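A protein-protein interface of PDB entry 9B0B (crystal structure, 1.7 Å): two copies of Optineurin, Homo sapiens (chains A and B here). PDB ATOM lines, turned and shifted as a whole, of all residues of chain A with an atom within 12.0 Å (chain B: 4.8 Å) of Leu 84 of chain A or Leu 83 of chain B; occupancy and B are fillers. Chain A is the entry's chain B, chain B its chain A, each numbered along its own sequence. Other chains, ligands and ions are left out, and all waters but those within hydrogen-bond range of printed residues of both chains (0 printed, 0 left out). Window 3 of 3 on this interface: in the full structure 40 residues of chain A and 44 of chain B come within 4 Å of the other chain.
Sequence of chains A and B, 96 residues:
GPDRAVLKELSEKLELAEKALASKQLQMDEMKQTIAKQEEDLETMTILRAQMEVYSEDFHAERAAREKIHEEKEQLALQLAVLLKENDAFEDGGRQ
Hydrophobic or aromatic side chains of chain B that line the printed part of chain A: Leu 80, Leu 83 and Leu 84. Printed residues of chain A that touch a printed residue of chain B: Leu 76, Gln 79, Leu 80, Leu 83 and Leu 84. Along chain A the printed residues that touch a printed residue of chain B span positions 76 to 84.
OE1 of Gln 75 of chain A sits at hydrogen-bond distance from NE2 of Gln 79 of chain A (2.4 Å). The backbone carbonyl oxygen (O) of Leu 83 of chain B lies close to the side-chain amide oxygen (OD1) of Asn 87 of chain B (2.9 Å).
CD2 of Leu 76 of chain A touches CD2 of Leu 80 of chain B, 3.9 Å away. Gln 79 of chain A touches Leu 80 of chain B (CB to CD2, 3.8 Å). Leu 80 of chain A touches Gln 79 of chain B. CD1 of Leu 80 of chain A touches CD2 of Leu 83 of chain B, 3.8 Å away. Leu 83 of chain A touches Leu 80 of chain B. Leu 83 of chain A touches Leu 83 of chain B (CB to CD2, 3.9 Å). CD1 of Leu 83 of chain A touches CD2 of Leu 84 of chain B, 3.6 Å away. Leu 83 of chain B touches Leu 84 of chain A.
Gln 79 of chain A touches Leu 80 of chain B, and with the chains exchanged Leu 80 of chain A touches Gln 79 of chain B. Leu 80 of chain A touches Leu 83 of chain B, and with the chains exchanged Leu 83 of chain A touches Leu 80 of chain B. Leu 83 of chain A touches its own counterpart, Leu 83 of chain B. Leu 83 of chain A touches Leu 84 of chain B, and with the chains exchanged Leu 84 of chain A touches Leu 83 of chain B. 7 positions are printed for both chains. Of the 8 pairs that touch across the chains among the printed residues, 7 have their exchanged pair printed and touching as well.
Printed residues of chain B within 4 Å of Gln 79 of chain A: Leu 80. Printed residues of chain B within 4 Å of Leu 83 of chain A: Leu 80, Leu 83 and Leu 84. Of the printed residues of chain A, Gln 79 of chain B touches Leu 80. Leu 80 of chain B touches three residues of chain A. No residue of chain A comes within 4 Å of Ala 81 of chain B. Leu 83 of chain B touches just these residues of chain A: Leu 80, Leu 83 and Leu 84. Leu 84 of chain B touches just one residue of chain A: Leu 83 (3.6 Å). Lys 85 of chain B touches none of the printed residues of chain A. No residue of chain A comes within 4 Å of Asn 87 of chain B. The nearest printed residue of chain B that does not touch Leu 84 of chain A is Gln 79 of chain B (6.4 Å). The nearest printed residue of chain B that does not touch Leu 80 of chain A is Leu 80 of chain B (4.1 Å).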
ATOM      1  N   GLN A  75      -8.099  -6.753 -20.098  1.00  0.00           N
ATOM      2  CA  GLN A  75      -7.887  -8.185 -20.289  1.00  0.00           C
ATOM      3  C   GLN A  75      -8.968  -8.796 -21.196  1.00  0.00           C
ATOM      4  O   GLN A  75      -8.661  -9.557 -22.125  1.00  0.00           O
ATOM      5  CB  GLN A  75      -7.824  -8.888 -18.934  1.00  0.00           C
ATOM      6  CG  GLN A  75      -8.040 -10.452 -19.003  1.00  0.00           C
ATOM      7  CD  GLN A  75      -6.873 -11.303 -19.675  1.00  0.00           C
ATOM      8  OE1 GLN A  75      -7.115 -12.162 -20.552  1.00  0.00           O
ATOM      9  NE2 GLN A  75      -5.689 -11.124 -19.204  1.00  0.00           N
ATOM     10  N   LEU A  76     -10.236  -8.462 -20.969  1.00  0.00           N
ATOM     11  CA  LEU A  76     -11.281  -8.990 -21.863  1.00  0.00           C
ATOM     12  C   LEU A  76     -11.087  -8.474 -23.278  1.00  0.00           C
ATOM     13  O   LEU A  76     -11.327  -9.190 -24.279  1.00  0.00           O
ATOM     14  CB  LEU A  76     -12.655  -8.603 -21.345  1.00  0.00           C
ATOM     15  CG  LEU A  76     -12.984  -9.313 -20.036  1.00  0.00           C
ATOM     16  CD1 LEU A  76     -14.383  -8.869 -19.530  1.00  0.00           C
ATOM     17  CD2 LEU A  76     -12.958 -10.816 -20.206  1.00  0.00           C
ATOM     18  N   ALA A  77     -10.696  -7.196 -23.406  1.00  0.00           N
ATOM     19  CA  ALA A  77     -10.554  -6.626 -24.740  1.00  0.00           C
ATOM     20  C   ALA A  77      -9.466  -7.369 -25.507  1.00  0.00           C
ATOM     21  O   ALA A  77      -9.538  -7.530 -26.743  1.00  0.00           O
ATOM     22  CB  ALA A  77     -10.223  -5.130 -24.656  1.00  0.00           C
ATOM     23  N   LEU A  78      -8.415  -7.745 -24.791  1.00  0.00           N
ATOM     24  CA  LEU A  78      -7.307  -8.487 -25.400  1.00  0.00           C
ATOM     25  C   LEU A  78      -7.775  -9.854 -25.880  1.00  0.00           C
ATOM     26  O   LEU A  78      -7.504 -10.257 -27.022  1.00  0.00           O
ATOM     27  CB  LEU A  78      -6.181  -8.648 -24.364  1.00  0.00           C
ATOM     28  CG  LEU A  78      -4.977  -9.565 -24.737  1.00  0.00           C
ATOM     29  CD1 LEU A  78      -4.256  -9.077 -25.998  1.00  0.00           C
ATOM     30  CD2 LEU A  78      -4.054  -9.757 -23.500  1.00  0.00           C
ATOM     31  N   GLN A  79      -8.522 -10.569 -25.028  1.00  0.00           N
ATOM     32  CA  GLN A  79      -9.039 -11.891 -25.436  1.00  0.00           C
ATOM     33  C   GLN A  79      -9.869 -11.759 -26.684  1.00  0.00           C
ATOM     34  O   GLN A  79      -9.790 -12.595 -27.593  1.00  0.00           O
ATOM     35  CB  GLN A  79      -9.909 -12.512 -24.322  1.00  0.00           C
ATOM     36  CG  GLN A  79      -9.205 -12.781 -22.978  1.00  0.00           C
ATOM     37  CD  GLN A  79      -8.128 -13.881 -23.095  1.00  0.00           C
ATOM     38  OE1 GLN A  79      -8.133 -14.668 -24.046  1.00  0.00           O
ATOM     39  NE2 GLN A  79      -7.309 -13.982 -22.108  1.00  0.00           N
ATOM     40  N   LEU A  80     -10.727 -10.735 -26.728  1.00  0.00           N
ATOM     41  CA  LEU A  80     -11.554 -10.546 -27.902  1.00  0.00           C
ATOM     42  C   LEU A  80     -10.676 -10.280 -29.122  1.00  0.00           C
ATOM     43  O   LEU A  80     -10.938 -10.813 -30.225  1.00  0.00           O
ATOM     44  CB  LEU A  80     -12.532  -9.403 -27.640  1.00  0.00           C
ATOM     45  CG  LEU A  80     -13.793  -9.065 -28.431  1.00  0.00           C
ATOM     46  CD1 LEU A  80     -14.763 -10.271 -28.455  1.00  0.00           C
ATOM     47  CD2 LEU A  80     -14.468  -7.903 -27.692  1.00  0.00           C
ATOM     48  N   ALA A  81      -9.637  -9.434 -28.939  1.00  0.00           N
ATOM     49  CA  ALA A  81      -8.760  -9.091 -30.060  1.00  0.00           C
ATOM     50  C   ALA A  81      -8.052 -10.338 -30.574  1.00  0.00           C
ATOM     51  O   ALA A  81      -7.919 -10.534 -31.789  1.00  0.00           O
ATOM     52  CB  ALA A  81      -7.735  -8.033 -29.631  1.00  0.00           C
ATOM     53  N   VAL A  82      -7.607 -11.200 -29.660  1.00  0.00           N
ATOM     54  CA  VAL A  82      -6.967 -12.441 -30.075  1.00  0.00           C
ATOM     55  C   VAL A  82      -7.952 -13.270 -30.888  1.00  0.00           C
ATOM     56  O   VAL A  82      -7.601 -13.830 -31.935  1.00  0.00           O
ATOM     57  CB  VAL A  82      -6.424 -13.230 -28.861  1.00  0.00           C
ATOM     58  CG1 VAL A  82      -6.040 -14.715 -29.308  1.00  0.00           C
ATOM     59  CG2 VAL A  82      -5.274 -12.504 -28.147  1.00  0.00           C
ATOM     60  N   LEU A  83      -9.208 -13.355 -30.447  1.00  0.00           N
ATOM     61  CA  LEU A  83     -10.144 -14.204 -31.167  1.00  0.00           C
ATOM     62  C   LEU A  83     -10.521 -13.618 -32.519  1.00  0.00           C
ATOM     63  O   LEU A  83     -10.792 -14.366 -33.466  1.00  0.00           O
ATOM     64  CB  LEU A  83     -11.412 -14.472 -30.374  1.00  0.00           C
ATOM     65  CG  LEU A  83     -11.181 -15.355 -29.113  1.00  0.00           C
ATOM     66  CD1 LEU A  83     -12.508 -15.708 -28.552  1.00  0.00           C
ATOM     67  CD2 LEU A  83     -10.333 -16.602 -29.382  1.00  0.00           C
ATOM     68  N   LEU A  84     -10.645 -12.290 -32.603  1.00  0.00           N
ATOM     69  CA  LEU A  84     -11.098 -11.713 -33.849  1.00  0.00           C
ATOM     70  C   LEU A  84      -9.987 -11.599 -34.887  1.00  0.00           C
ATOM     71  O   LEU A  84     -10.289 -11.271 -36.038  1.00  0.00           O
ATOM     72  CB  LEU A  84     -11.770 -10.373 -33.576  1.00  0.00           C
ATOM     73  CG  LEU A  84     -13.109 -10.498 -32.849  1.00  0.00           C
ATOM     74  CD1 LEU A  84     -13.666  -9.151 -32.384  1.00  0.00           C
ATOM     75  CD2 LEU A  84     -14.095 -11.177 -33.792  1.00  0.00           C
ATOM     76  N   LYS A  85      -8.735 -11.878 -34.518  1.00  0.00           N
ATOM     77  CA  LYS A  85      -7.590 -11.724 -35.427  1.00  0.00           C
ATOM     78  C   LYS A  85      -7.423 -12.933 -36.346  1.00  0.00           C
ATOM     79  O   LYS A  85      -8.404 -13.595 -36.707  1.00  0.00           O
ATOM     80  CB  LYS A  85      -6.310 -11.497 -34.648  1.00  0.00           C
ATOM     81  N   GLN B  79     -19.998  -9.806 -25.187  1.00  0.00           N
ATOM     82  CA  GLN B  79     -19.555 -10.018 -26.571  1.00  0.00           C
ATOM     83  C   GLN B  79     -18.656 -11.231 -26.674  1.00  0.00           C
ATOM     84  O   GLN B  79     -18.767 -12.018 -27.621  1.00  0.00           O
ATOM     85  CB  GLN B  79     -18.809  -8.798 -27.119  1.00  0.00           C
ATOM     86  CG  GLN B  79     -19.600  -7.536 -27.137  1.00  0.00           C
ATOM     87  CD  GLN B  79     -18.773  -6.331 -27.553  1.00  0.00           C
ATOM     88  OE1 GLN B  79     -19.225  -5.195 -27.414  1.00  0.00           O
ATOM     89  NE2 GLN B  79     -17.574  -6.567 -28.073  1.00  0.00           N
ATOM     90  N   LEU B  80     -17.730 -11.372 -25.739  1.00  0.00           N
ATOM     91  CA  LEU B  80     -16.808 -12.497 -25.748  1.00  0.00           C
ATOM     92  C   LEU B  80     -17.548 -13.826 -25.545  1.00  0.00           C
ATOM     93  O   LEU B  80     -17.263 -14.814 -26.237  1.00  0.00           O
ATOM     94  CB  LEU B  80     -15.725 -12.284 -24.663  1.00  0.00           C
ATOM     95  CG  LEU B  80     -14.548 -13.249 -24.575  1.00  0.00           C
ATOM     96  CD1 LEU B  80     -13.784 -13.290 -25.904  1.00  0.00           C
ATOM     97  CD2 LEU B  80     -13.553 -12.905 -23.415  1.00  0.00           C
ATOM     98  N   ALA B  81     -18.483 -13.867 -24.596  1.00  0.00           N
ATOM     99  CA  ALA B  81     -19.206 -15.112 -24.336  1.00  0.00           C
ATOM    100  C   ALA B  81     -20.001 -15.528 -25.572  1.00  0.00           C
ATOM    101  O   ALA B  81     -20.057 -16.719 -25.930  1.00  0.00           O
ATOM    102  CB  ALA B  81     -20.135 -14.942 -23.119  1.00  0.00           C
ATOM    103  N   VAL B  82     -20.623 -14.554 -26.239  1.00  0.00           N
ATOM    104  CA  VAL B  82     -21.403 -14.831 -27.451  1.00  0.00           C
ATOM    105  C   VAL B  82     -20.491 -15.368 -28.557  1.00  0.00           C
ATOM    106  O   VAL B  82     -20.872 -16.278 -29.342  1.00  0.00           O
ATOM    107  CB  VAL B  82     -22.139 -13.554 -27.903  1.00  0.00           C
ATOM    108  CG1 VAL B  82     -22.677 -13.696 -29.361  1.00  0.00           C
ATOM    109  CG2 VAL B  82     -23.304 -13.243 -26.987  1.00  0.00           C
ATOM    110  N   LEU B  83     -19.328 -14.739 -28.709  1.00  0.00           N
ATOM    111  CA  LEU B  83     -18.398 -15.150 -29.777  1.00  0.00           C
ATOM    112  C   LEU B  83     -17.891 -16.571 -29.537  1.00  0.00           C
ATOM    113  O   LEU B  83     -17.793 -17.380 -30.473  1.00  0.00           O
ATOM    114  CB  LEU B  83     -17.230 -14.177 -29.846  1.00  0.00           C
ATOM    115  CG  LEU B  83     -16.188 -14.382 -30.934  1.00  0.00           C
ATOM    116  CD1 LEU B  83     -16.857 -14.226 -32.279  1.00  0.00           C
ATOM    117  CD2 LEU B  83     -15.102 -13.278 -30.761  1.00  0.00           C
ATOM    118  N   LEU B  84     -17.669 -16.922 -28.278  1.00  0.00           N
ATOM    119  CA  LEU B  84     -17.228 -18.273 -27.941  1.00  0.00           C
ATOM    120  C   LEU B  84     -18.349 -19.267 -28.158  1.00  0.00           C
ATOM    121  O   LEU B  84     -18.105 -20.393 -28.611  1.00  0.00           O
ATOM    122  CB  LEU B  84     -16.800 -18.330 -26.474  1.00  0.00           C
ATOM    123  CG  LEU B  84     -15.528 -17.594 -26.145  1.00  0.00           C
ATOM    124  CD1 LEU B  84     -15.330 -17.490 -24.619  1.00  0.00           C
ATOM    125  CD2 LEU B  84     -14.304 -18.310 -26.822  1.00  0.00           C
ATOM    126  N   LYS B  85     -19.576 -18.887 -27.802  1.00  0.00           N
ATOM    127  CA  LYS B  85     -20.692 -19.815 -27.926  1.00  0.00           C
ATOM    128  C   LYS B  85     -21.078 -19.979 -29.384  1.00  0.00           C
ATOM    129  O   LYS B  85     -21.374 -21.091 -29.830  1.00  0.00           O
ATOM    130  CB  LYS B  85     -21.876 -19.322 -27.085  1.00  0.00           C
ATOM    131  CG  LYS B  85     -23.104 -20.246 -27.058  1.00  0.00           C
ATOM    132  CD  LYS B  85     -22.773 -21.575 -26.432  1.00  0.00           C
ATOM    133  CE  LYS B  85     -24.024 -22.262 -25.915  1.00  0.00           C
ATOM    134  NZ  LYS B  85     -25.091 -22.368 -26.935  1.00  0.00           N
ATOM    135  N   GLU B  86     -21.059 -18.887 -30.149  1.00  0.00           N
ATOM    136  CA  GLU B  86     -21.173 -18.990 -31.604  1.00  0.00           C
ATOM    137  C   GLU B  86     -20.160 -19.961 -32.210  1.00  0.00           C
ATOM    138  O   GLU B  86     -20.437 -20.580 -33.239  1.00  0.00           O
ATOM    139  CB  GLU B  86     -20.985 -17.628 -32.245  1.00  0.00           C
ATOM    140  CG  GLU B  86     -22.221 -16.797 -32.218  1.00  0.00           C
ATOM    141  CD  GLU B  86     -22.017 -15.501 -32.964  1.00  0.00           C
ATOM    142  OE1 GLU B  86     -20.858 -15.023 -32.976  1.00  0.00           O
ATOM    143  OE2 GLU B  86     -23.001 -14.971 -33.531  1.00  0.00           O
ATOM    144  N   ASN B  87     -18.982 -20.097 -31.605  1.00  0.00           N
ATOM    145  CA  ASN B  87     -17.955 -21.012 -32.088  1.00  0.00           C
ATOM    146  C   ASN B  87     -17.955 -22.351 -31.341  1.00  0.00           C
ATOM    147  O   ASN B  87     -16.961 -23.085 -31.402  1.00  0.00           O
ATOM    148  CB  ASN B  87     -16.571 -20.356 -31.988  1.00  0.00           C
ATOM    149  CG  ASN B  87     -16.320 -19.351 -33.098  1.00  0.00           C
ATOM    150  OD1 ASN B  87     -16.880 -18.251 -33.097  1.00  0.00           O
ATOM    151  ND2 ASN B  87     -15.459 -19.721 -34.051  1.00  0.00           N
